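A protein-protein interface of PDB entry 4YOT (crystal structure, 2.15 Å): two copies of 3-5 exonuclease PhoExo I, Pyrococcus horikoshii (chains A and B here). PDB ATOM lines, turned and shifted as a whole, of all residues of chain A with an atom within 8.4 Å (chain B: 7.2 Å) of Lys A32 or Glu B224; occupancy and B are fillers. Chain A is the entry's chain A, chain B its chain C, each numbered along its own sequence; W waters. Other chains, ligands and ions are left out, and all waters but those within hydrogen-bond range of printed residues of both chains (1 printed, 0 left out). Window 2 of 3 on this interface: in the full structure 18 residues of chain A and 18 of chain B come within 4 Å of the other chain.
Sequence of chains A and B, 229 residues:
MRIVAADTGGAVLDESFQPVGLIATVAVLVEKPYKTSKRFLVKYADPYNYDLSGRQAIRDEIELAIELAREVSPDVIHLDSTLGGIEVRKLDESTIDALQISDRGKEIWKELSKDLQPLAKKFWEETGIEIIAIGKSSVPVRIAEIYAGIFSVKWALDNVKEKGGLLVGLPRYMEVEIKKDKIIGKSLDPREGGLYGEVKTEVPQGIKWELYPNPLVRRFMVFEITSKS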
ATOM      1  N   MET A   1      14.981  28.197  11.280  1.00  0.00           N
ATOM      2  CA  MET A   1      16.135  27.645  11.988  1.00  0.00           C
ATOM      3  C   MET A   1      17.415  27.866  11.182  1.00  0.00           C
ATOM      4  O   MET A   1      17.424  27.714   9.964  1.00  0.00           O
ATOM      5  CB  MET A   1      15.929  26.152  12.265  1.00  0.00           C
ATOM      6  CG  MET A   1      16.895  25.575  13.279  1.00  0.00           C
ATOM      7  SD  MET A   1      16.754  23.787  13.465  1.00  0.00           S
ATOM      8  CE  MET A   1      15.077  23.627  14.055  1.00  0.00           C
ATOM      9  N   ARG A   2      18.485  28.252  11.867  1.00  0.00           N
ATOM     10  CA  ARG A   2      19.780  28.433  11.219  1.00  0.00           C
ATOM     11  C   ARG A   2      20.767  27.424  11.784  1.00  0.00           C
ATOM     12  O   ARG A   2      20.981  27.361  13.002  1.00  0.00           O
ATOM     13  CB  ARG A   2      20.289  29.864  11.414  1.00  0.00           C
ATOM     14  CG  ARG A   2      19.370  30.909  10.801  1.00  0.00           C
ATOM     15  CD  ARG A   2      19.769  32.328  11.172  1.00  0.00           C
ATOM     16  NE  ARG A   2      20.994  32.763  10.504  1.00  0.00           N
ATOM     17  CZ  ARG A   2      22.136  33.016  11.139  1.00  0.00           C
ATOM     18  NH1 ARG A   2      23.203  33.412  10.462  1.00  0.00           N
ATOM     19  NH2 ARG A   2      22.209  32.881  12.457  1.00  0.00           N
ATOM     20  N   ILE A   3      21.362  26.633  10.892  1.00  0.00           N
ATOM     21  CA  ILE A   3      22.198  25.504  11.288  1.00  0.00           C
ATOM     22  C   ILE A   3      23.612  25.566  10.695  1.00  0.00           C
ATOM     23  O   ILE A   3      23.783  25.815   9.495  1.00  0.00           O
ATOM     24  CB  ILE A   3      21.551  24.176  10.849  1.00  0.00           C
ATOM     25  CG1 ILE A   3      20.117  24.083  11.381  1.00  0.00           C
ATOM     26  CG2 ILE A   3      22.391  22.983  11.304  1.00  0.00           C
ATOM     27  CD1 ILE A   3      19.258  23.040  10.680  1.00  0.00           C
ATOM     28  N   LEU A  29      26.942  27.176   6.739  1.00  0.00           N
ATOM     29  CA  LEU A  29      25.748  27.731   7.360  1.00  0.00           C
ATOM     30  C   LEU A  29      24.595  27.421   6.426  1.00  0.00           C
ATOM     31  O   LEU A  29      24.634  27.781   5.244  1.00  0.00           O
ATOM     32  CB  LEU A  29      25.873  29.243   7.558  1.00  0.00           C
ATOM     33  CG  LEU A  29      24.603  30.022   7.921  1.00  0.00           C
ATOM     34  CD1 LEU A  29      24.042  29.592   9.269  1.00  0.00           C
ATOM     35  CD2 LEU A  29      24.852  31.525   7.902  1.00  0.00           C
ATOM     36  N   VAL A  30      23.582  26.733   6.944  1.00  0.00           N
ATOM     37  CA  VAL A  30      22.399  26.417   6.153  1.00  0.00           C
ATOM     38  C   VAL A  30      21.154  27.086   6.727  1.00  0.00           C
ATOM     39  O   VAL A  30      20.843  26.933   7.911  1.00  0.00           O
ATOM     40  CB  VAL A  30      22.162  24.898   6.061  1.00  0.00           C
ATOM     41  CG1 VAL A  30      20.923  24.605   5.233  1.00  0.00           C
ATOM     42  CG2 VAL A  30      23.382  24.200   5.468  1.00  0.00           C
ATOM     43  N   GLU A  31      20.458  27.839   5.879  1.00  0.00           N
ATOM     44  CA  GLU A  31      19.191  28.459   6.246  1.00  0.00           C
ATOM     45  C   GLU A  31      18.094  27.988   5.298  1.00  0.00           C
ATOM     46  O   GLU A  31      18.372  27.388   4.255  1.00  0.00           O
ATOM     47  CB  GLU A  31      19.296  29.984   6.171  1.00  0.00           C
ATOM     48  CG  GLU A  31      20.245  30.608   7.178  1.00  0.00           C
ATOM     49  CD  GLU A  31      20.361  32.111   7.013  1.00  0.00           C
ATOM     50  OE1 GLU A  31      21.328  32.567   6.370  1.00  0.00           O
ATOM     51  OE2 GLU A  31      19.482  32.835   7.526  1.00  0.00           O
ATOM     52  N   LYS A  32      16.850  28.260   5.673  1.00  0.00           N
ATOM     53  CA  LYS A  32      15.696  28.003   4.819  1.00  0.00           C
ATOM     54  C   LYS A  32      15.974  28.567   3.427  1.00  0.00           C
ATOM     55  O   LYS A  32      16.495  29.679   3.304  1.00  0.00           O
ATOM     56  CB  LYS A  32      14.474  28.685   5.436  1.00  0.00           C
ATOM     57  CG  LYS A  32      13.144  28.323   4.816  1.00  0.00           C
ATOM     58  CD  LYS A  32      12.031  28.986   5.594  1.00  0.00           C
ATOM     59  CE  LYS A  32      10.707  28.830   4.894  1.00  0.00           C
ATOM     60  NZ  LYS A  32       9.633  29.489   5.678  1.00  0.00           N
ATOM     61  N   PRO A  33      15.638  27.811   2.368  1.00  0.00           N
ATOM     62  CA  PRO A  33      14.901  26.541   2.335  1.00  0.00           C
ATOM     63  C   PRO A  33      15.753  25.278   2.468  1.00  0.00           C
ATOM     64  O   PRO A  33      15.291  24.211   2.063  1.00  0.00           O
ATOM     65  CB  PRO A  33      14.245  26.571   0.952  1.00  0.00           C
ATOM     66  CG  PRO A  33      15.221  27.314   0.111  1.00  0.00           C
ATOM     67  CD  PRO A  33      15.871  28.339   1.010  1.00  0.00           C
ATOM     68  N   TYR A  34      16.958  25.392   3.019  1.00  0.00           N
ATOM     69  CA  TYR A  34      17.744  24.217   3.398  1.00  0.00           C
ATOM     70  C   TYR A  34      18.123  23.339   2.197  1.00  0.00           C
ATOM     71  O   TYR A  34      18.066  22.115   2.282  1.00  0.00           O
ATOM     72  CB  TYR A  34      16.995  23.379   4.451  1.00  0.00           C
ATOM     73  CG  TYR A  34      16.408  24.196   5.592  1.00  0.00           C
ATOM     74  CD1 TYR A  34      17.218  24.707   6.594  1.00  0.00           C
ATOM     75  CD2 TYR A  34      15.042  24.444   5.665  1.00  0.00           C
ATOM     76  CE1 TYR A  34      16.684  25.450   7.637  1.00  0.00           C
ATOM     77  CE2 TYR A  34      14.498  25.180   6.702  1.00  0.00           C
ATOM     78  CZ  TYR A  34      15.323  25.683   7.681  1.00  0.00           C
ATOM     79  OH  TYR A  34      14.788  26.422   8.712  1.00  0.00           O
ATOM     80  N   LYS A  35      18.505  23.967   1.087  1.00  0.00           N
ATOM     81  CA  LYS A  35      18.907  23.230  -0.111  1.00  0.00           C
ATOM     82  C   LYS A  35      20.374  23.455  -0.439  1.00  0.00           C
ATOM     83  O   LYS A  35      20.998  22.642  -1.121  1.00  0.00           O
ATOM     84  CB  LYS A  35      18.057  23.645  -1.308  1.00  0.00           C
ATOM     85  CG  LYS A  35      16.635  23.126  -1.276  1.00  0.00           C
ATOM     86  CD  LYS A  35      15.808  23.757  -2.394  1.00  0.00           C
ATOM     87  CE  LYS A  35      14.449  23.089  -2.518  1.00  0.00           C
ATOM     88  NZ  LYS A  35      13.587  23.712  -3.570  1.00  0.00           N
ATOM     89  N   THR A  36      20.919  24.569   0.033  1.00  0.00           N
ATOM     90  CA  THR A  36      22.311  24.891  -0.246  1.00  0.00           C
ATOM     91  C   THR A  36      22.921  25.722   0.885  1.00  0.00           C
ATOM     92  O   THR A  36      22.326  25.854   1.961  1.00  0.00           O
ATOM     93  CB  THR A  36      22.442  25.621  -1.597  1.00  0.00           C
ATOM     94  OG1 THR A  36      23.825  25.733  -1.959  1.00  0.00           O
ATOM     95  CG2 THR A  36      21.798  27.006  -1.525  1.00  0.00           C
ATOM     96  N   LYS A  38      25.401  29.455   1.417  1.00  0.00           N
ATOM     97  CA  LYS A  38      26.028  30.607   0.772  1.00  0.00           C
ATOM     98  C   LYS A  38      27.213  31.099   1.599  1.00  0.00           C
ATOM     99  O   LYS A  38      27.926  32.021   1.200  1.00  0.00           O
ATOM    100  CB  LYS A  38      25.008  31.734   0.587  1.00  0.00           C
ATOM    101  CG  LYS A  38      23.746  31.328  -0.169  1.00  0.00           C
ATOM    102  CD  LYS A  38      24.039  31.033  -1.634  1.00  0.00           C
ATOM    103  CE  LYS A  38      22.775  30.641  -2.384  1.00  0.00           C
ATOM    104  NZ  LYS A  38      23.007  30.571  -3.854  1.00  0.00           N
ATOM    105  N   GLU B  15       7.373  24.929  14.778  1.00  0.00           N
ATOM    106  CA  GLU B  15       8.300  25.780  14.035  1.00  0.00           C
ATOM    107  C   GLU B  15       9.727  25.224  13.994  1.00  0.00           C
ATOM    108  O   GLU B  15      10.522  25.620  13.139  1.00  0.00           O
ATOM    109  CB  GLU B  15       8.302  27.206  14.598  1.00  0.00           C
ATOM    110  CG  GLU B  15       7.725  28.258  13.652  1.00  0.00           C
ATOM    111  CD  GLU B  15       6.211  28.332  13.694  1.00  0.00           C
ATOM    112  OE1 GLU B  15       5.641  28.336  14.806  1.00  0.00           O
ATOM    113  OE2 GLU B  15       5.589  28.394  12.613  1.00  0.00           O
ATOM    114  N   PHE B  17      10.320  21.993  13.536  1.00  0.00           N
ATOM    115  CA  PHE B  17      10.214  20.760  12.745  1.00  0.00           C
ATOM    116  C   PHE B  17       9.981  19.497  13.560  1.00  0.00           C
ATOM    117  O   PHE B  17      10.058  18.386  13.028  1.00  0.00           O
ATOM    118  CB  PHE B  17      11.422  20.582  11.819  1.00  0.00           C
ATOM    119  CG  PHE B  17      11.744  21.802  11.027  1.00  0.00           C
ATOM    120  CD1 PHE B  17      10.890  22.238  10.022  1.00  0.00           C
ATOM    121  CD2 PHE B  17      12.893  22.526  11.295  1.00  0.00           C
ATOM    122  CE1 PHE B  17      11.181  23.375   9.298  1.00  0.00           C
ATOM    123  CE2 PHE B  17      13.194  23.661  10.576  1.00  0.00           C
ATOM    124  CZ  PHE B  17      12.339  24.088   9.573  1.00  0.00           C
ATOM    125  N   ALA B 156      -4.346  21.051   5.456  1.00  0.00           N
ATOM    126  CA  ALA B 156      -3.625  22.275   5.784  1.00  0.00           C
ATOM    127  C   ALA B 156      -4.214  23.502   5.091  1.00  0.00           C
ATOM    128  O   ALA B 156      -4.287  24.576   5.686  1.00  0.00           O
ATOM    129  CB  ALA B 156      -2.159  22.129   5.439  1.00  0.00           C
ATOM    130  N   GLY B 165      -0.690  29.910  10.362  1.00  0.00           N
ATOM    131  CA  GLY B 165       0.484  29.331   9.730  1.00  0.00           C
ATOM    132  C   GLY B 165       0.625  27.858  10.058  1.00  0.00           C
ATOM    133  O   GLY B 165       0.374  27.443  11.190  1.00  0.00           O
ATOM    134  N   LEU B 166       1.029  27.061   9.075  1.00  0.00           N
ATOM    135  CA  LEU B 166       1.099  25.618   9.271  1.00  0.00           C
ATOM    136  C   LEU B 166       2.328  24.964   8.639  1.00  0.00           C
ATOM    137  O   LEU B 166       2.704  25.277   7.508  1.00  0.00           O
ATOM    138  CB  LEU B 166      -0.171  24.947   8.740  1.00  0.00           C
ATOM    139  CG  LEU B 166      -1.438  25.102   9.582  1.00  0.00           C
ATOM    140  CD1 LEU B 166      -2.662  24.594   8.839  1.00  0.00           C
ATOM    141  CD2 LEU B 166      -1.268  24.360  10.892  1.00  0.00           C
ATOM    142  N   LEU B 167       2.944  24.056   9.390  1.00  0.00           N
ATOM    143  CA  LEU B 167       4.013  23.209   8.874  1.00  0.00           C
ATOM    144  C   LEU B 167       3.519  21.772   8.813  1.00  0.00           C
ATOM    145  O   LEU B 167       3.160  21.186   9.837  1.00  0.00           O
ATOM    146  CB  LEU B 167       5.254  23.294   9.765  1.00  0.00           C
ATOM    147  CG  LEU B 167       6.027  24.607   9.705  1.00  0.00           C
ATOM    148  CD1 LEU B 167       7.242  24.582  10.607  1.00  0.00           C
ATOM    149  CD2 LEU B 167       6.455  24.852   8.290  1.00  0.00           C
ATOM    150  N   VAL B 168       3.474  21.214   7.610  1.00  0.00           N
ATOM    151  CA  VAL B 168       3.080  19.822   7.439  1.00  0.00           C
ATOM    152  C   VAL B 168       4.276  18.980   7.015  1.00  0.00           C
ATOM    153  O   VAL B 168       4.903  19.250   5.991  1.00  0.00           O
ATOM    154  CB  VAL B 168       1.950  19.667   6.403  1.00  0.00           C
ATOM    155  CG1 VAL B 168       1.652  18.201   6.162  1.00  0.00           C
ATOM    156  CG2 VAL B 168       0.703  20.382   6.880  1.00  0.00           C
ATOM    157  N   LYS B 208       0.202  31.854   0.920  1.00  0.00           N
ATOM    158  CA  LYS B 208       1.453  31.559   0.244  1.00  0.00           C
ATOM    159  C   LYS B 208       1.905  30.210   0.775  1.00  0.00           C
ATOM    160  O   LYS B 208       1.735  29.921   1.963  1.00  0.00           O
ATOM    161  CB  LYS B 208       2.506  32.622   0.563  1.00  0.00           C
ATOM    162  CG  LYS B 208       1.930  34.013   0.795  1.00  0.00           C
ATOM    163  CD  LYS B 208       3.011  35.032   1.127  1.00  0.00           C
ATOM    164  CE  LYS B 208       3.813  35.408  -0.106  1.00  0.00           C
ATOM    165  NZ  LYS B 208       4.829  36.446   0.201  1.00  0.00           N
ATOM    166  N   TRP B 209       2.460  29.377  -0.096  1.00  0.00           N
ATOM    167  CA  TRP B 209       2.953  28.079   0.341  1.00  0.00           C
ATOM    168  C   TRP B 209       4.340  27.800  -0.210  1.00  0.00           C
ATOM    169  O   TRP B 209       4.804  28.472  -1.134  1.00  0.00           O
ATOM    170  CB  TRP B 209       2.001  26.953  -0.050  1.00  0.00           C
ATOM    171  CG  TRP B 209       1.891  26.749  -1.520  1.00  0.00           C
ATOM    172  CD1 TRP B 209       2.626  25.895  -2.286  1.00  0.00           C
ATOM    173  CD2 TRP B 209       0.980  27.405  -2.407  1.00  0.00           C
ATOM    174  NE1 TRP B 209       2.230  25.981  -3.600  1.00  0.00           N
ATOM    175  CE2 TRP B 209       1.220  26.903  -3.700  1.00  0.00           C
ATOM    176  CE3 TRP B 209      -0.017  28.369  -2.234  1.00  0.00           C
ATOM    177  CZ2 TRP B 209       0.499  27.335  -4.815  1.00  0.00           C
ATOM    178  CZ3 TRP B 209      -0.728  28.796  -3.337  1.00  0.00           C
ATOM    179  CH2 TRP B 209      -0.467  28.280  -4.611  1.00  0.00           C
ATOM    180  N   GLU B 210       4.992  26.796   0.360  1.00  0.00           N
ATOM    181  CA  GLU B 210       6.360  26.476  -0.008  1.00  0.00           C
ATOM    182  C   GLU B 210       6.676  25.036   0.350  1.00  0.00           C
ATOM    183  O   GLU B 210       6.210  24.525   1.373  1.00  0.00           O
ATOM    184  CB  GLU B 210       7.323  27.408   0.722  1.00  0.00           C
ATOM    185  CG  GLU B 210       8.321  28.100  -0.179  1.00  0.00           C
ATOM    186  CD  GLU B 210       9.269  28.987   0.600  1.00  0.00           C
ATOM    187  OE1 GLU B 210      10.431  29.135   0.168  1.00  0.00           O
ATOM    188  OE2 GLU B 210       8.848  29.536   1.643  1.00  0.00           O
ATOM    189  N   LEU B 211       7.470  24.386  -0.494  1.00  0.00           N
ATOM    190  CA  LEU B 211       7.896  23.021  -0.244  1.00  0.00           C
ATOM    191  C   LEU B 211       9.416  23.007  -0.151  1.00  0.00           C
ATOM    192  O   LEU B 211      10.102  23.559  -1.014  1.00  0.00           O
ATOM    193  CB  LEU B 211       7.417  22.105  -1.367  1.00  0.00           C
ATOM    194  CG  LEU B 211       7.750  20.624  -1.214  1.00  0.00           C
ATOM    195  CD1 LEU B 211       6.990  20.041  -0.049  1.00  0.00           C
ATOM    196  CD2 LEU B 211       7.419  19.879  -2.485  1.00  0.00           C
ATOM    197  N   TYR B 212       9.945  22.403   0.908  1.00  0.00           N
ATOM    198  CA  TYR B 212      11.390  22.388   1.121  1.00  0.00           C
ATOM    199  C   TYR B 212      11.805  21.214   2.011  1.00  0.00           C
ATOM    200  O   TYR B 212      10.966  20.634   2.704  1.00  0.00           O
ATOM    201  CB  TYR B 212      11.874  23.728   1.703  1.00  0.00           C
ATOM    202  CG  TYR B 212      11.229  24.137   3.014  1.00  0.00           C
ATOM    203  CD1 TYR B 212      11.667  23.607   4.221  1.00  0.00           C
ATOM    204  CD2 TYR B 212      10.193  25.070   3.044  1.00  0.00           C
ATOM    205  CE1 TYR B 212      11.091  23.979   5.417  1.00  0.00           C
ATOM    206  CE2 TYR B 212       9.609  25.454   4.243  1.00  0.00           C
ATOM    207  CZ  TYR B 212      10.066  24.903   5.424  1.00  0.00           C
ATOM    208  OH  TYR B 212       9.503  25.267   6.624  1.00  0.00           O
ATOM    209  N   PRO B 213      13.097  20.840   1.972  1.00  0.00           N
ATOM    210  CA  PRO B 213      13.580  19.757   2.835  1.00  0.00           C
ATOM    211  C   PRO B 213      13.423  20.035   4.328  1.00  0.00           C
ATOM    212  O   PRO B 213      13.713  21.134   4.800  1.00  0.00           O
ATOM    213  CB  PRO B 213      15.074  19.692   2.501  1.00  0.00           C
ATOM    214  CG  PRO B 213      15.163  20.185   1.087  1.00  0.00           C
ATOM    215  CD  PRO B 213      14.120  21.271   0.999  1.00  0.00           C
ATOM    216  N   VAL B 222       8.904  19.252   3.733  1.00  0.00           N
ATOM    217  CA  VAL B 222       7.991  20.003   4.577  1.00  0.00           C
ATOM    218  C   VAL B 222       7.122  20.832   3.652  1.00  0.00           C
ATOM    219  O   VAL B 222       7.647  21.509   2.764  1.00  0.00           O
ATOM    220  CB  VAL B 222       8.758  20.968   5.507  1.00  0.00           C
ATOM    221  CG1 VAL B 222       7.807  21.966   6.150  1.00  0.00           C
ATOM    222  CG2 VAL B 222       9.549  20.199   6.574  1.00  0.00           C
ATOM    223  N   PHE B 223       5.805  20.762   3.834  1.00  0.00           N
ATOM    224  CA  PHE B 223       4.896  21.680   3.150  1.00  0.00           C
ATOM    225  C   PHE B 223       4.451  22.762   4.115  1.00  0.00           C
ATOM    226  O   PHE B 223       3.763  22.496   5.102  1.00  0.00           O
ATOM    227  CB  PHE B 223       3.673  20.963   2.570  1.00  0.00           C
ATOM    228  CG  PHE B 223       2.684  21.895   1.905  1.00  0.00           C
ATOM    229  CD1 PHE B 223       2.832  22.252   0.571  1.00  0.00           C
ATOM    230  CD2 PHE B 223       1.610  22.415   2.617  1.00  0.00           C
ATOM    231  CE1 PHE B 223       1.928  23.110  -0.040  1.00  0.00           C
ATOM    232  CE2 PHE B 223       0.701  23.279   2.013  1.00  0.00           C
ATOM    233  CZ  PHE B 223       0.866  23.626   0.686  1.00  0.00           C
ATOM    234  N   GLU B 224       4.845  23.987   3.807  1.00  0.00           N
ATOM    235  CA  GLU B 224       4.592  25.116   4.669  1.00  0.00           C
ATOM    236  C   GLU B 224       3.583  26.041   4.012  1.00  0.00           C
ATOM    237  O   GLU B 224       3.730  26.390   2.841  1.00  0.00           O
ATOM    238  CB  GLU B 224       5.901  25.857   4.898  1.00  0.00           C
ATOM    239  CG  GLU B 224       5.785  27.144   5.670  1.00  0.00           C
ATOM    240  CD  GLU B 224       7.131  27.797   5.843  1.00  0.00           C
ATOM    241  OE1 GLU B 224       7.559  28.515   4.916  1.00  0.00           O
ATOM    242  OE2 GLU B 224       7.772  27.581   6.892  1.00  0.00           O
ATOM    243  N   ILE B 225       2.564  26.438   4.765  1.00  0.00           N
ATOM    244  CA  ILE B 225       1.549  27.347   4.249  1.00  0.00           C
ATOM    245  C   ILE B 225       1.270  28.467   5.248  1.00  0.00           C
ATOM    246  O   ILE B 225       1.142  28.223   6.449  1.00  0.00           O
ATOM    247  CB  ILE B 225       0.252  26.588   3.872  1.00  0.00           C
ATOM    248  CG1 ILE B 225      -0.777  27.535   3.269  1.00  0.00           C
ATOM    249  CG2 ILE B 225      -0.337  25.856   5.065  1.00  0.00           C
ATOM    250  CD1 ILE B 225      -2.069  26.853   2.922  1.00  0.00           C
ATOM    251  N   THR B 226       1.205  29.699   4.751  1.00  0.00           N
ATOM    252  CA  THR B 226       0.957  30.861   5.604  1.00  0.00           C
ATOM    253  C   THR B 226      -0.147  31.750   5.030  1.00  0.00           C
ATOM    254  O   THR B 226      -0.478  31.655   3.847  1.00  0.00           O
ATOM    255  CB  THR B 226       2.231  31.711   5.796  1.00  0.00           C
ATOM    256  OG1 THR B 226       2.610  32.295   4.544  1.00  0.00           O
ATOM    257  CG2 THR B 226       3.378  30.860   6.324  1.00  0.00           C
HETATM  258  O   HOH W   1      11.469  22.369  -3.367  1.00  0.00           O
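The backbone NH (N) of Met A1 lies within hydrogen-bond range of the side-chain hydroxyl (OH) of Tyr A34, 3.1 Å away. The backbone carbonyl oxygen of Glu B224 sits at hydrogen-bond distance from the backbone NH of Glu B210, at 2.8 Å. The backbone NH (N) of Val B222 lies within hydrogen-bond range of the backbone carbonyl oxygen (O) of Tyr B212, 2.7 Å away. OH of Tyr B212 sits at hydrogen-bond distance from OE2 of Glu B224 (2.9 Å).
Hydrophobic or aromatic side chains of chain B that line the printed part of chain A: Phe B17, Tyr B212 and Pro B213.
The side-chain amino group (NZ) of Lys A32 lies within salt-bridge range of the side-chain carboxylate (OE1) of Glu B224.
Among the printed residues, pairs that only touch across the chains: Met A1 with Phe B17 (3.7 Å), Lys A32 with Glu B210 (3.8 Å), Lys A32 with Tyr B212 (3.6 Å), Pro A33 with Tyr B212 (3.5 Å), Pro A33 with Pro B213 (3.3 Å), Tyr A34 with Phe B17 (3.5 Å), Tyr A34 with Tyr B212 (3.8 Å), Tyr A34 with Pro B213 (3.7 Å) and Lys A35 with Pro B213 (3.9 Å).
No position is printed for both chains. Of the 10 pairs that touch across the chains among the printed residues, none has its exchanged pair printed and touching as well.
Water W1 bridges the side-chain amino group (NZ) of Lys A35 (2.5 Å) and the backbone carbonyl oxygen (O) of Leu B211 (3.0 Å).
Of chain B, only Glu B210 (3.8 Å), Tyr B212 (3.6 Å) and Glu B224 (2.4 Å) come within 4 Å of Lys A32. Glu B224 touches just one residue of chain A: Lys A32 (2.4 Å). Of the printed residues of chain A, Tyr B212 touches Lys A32 (3.6 Å), Pro A33 (3.5 Å) and Tyr A34 (3.8 Å). Of the printed residues of chain A, Glu B210 touches Lys A32. Of the printed residues of chain A, Phe B17 touches Met A1 (3.7 Å) and Tyr A34 (3.5 Å). Of the printed residues of chain B, Tyr A34 touches Phe B17 (3.5 Å), Tyr B212 (3.8 Å) and Pro B213 (3.7 Å). Arg A2 touches none of the printed residues of chain B. Ile A3 touches none of the printed residues of chain B. The nearest residue of chain B that does not touch Lys A32 is Leu B167 (6.2 Å).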
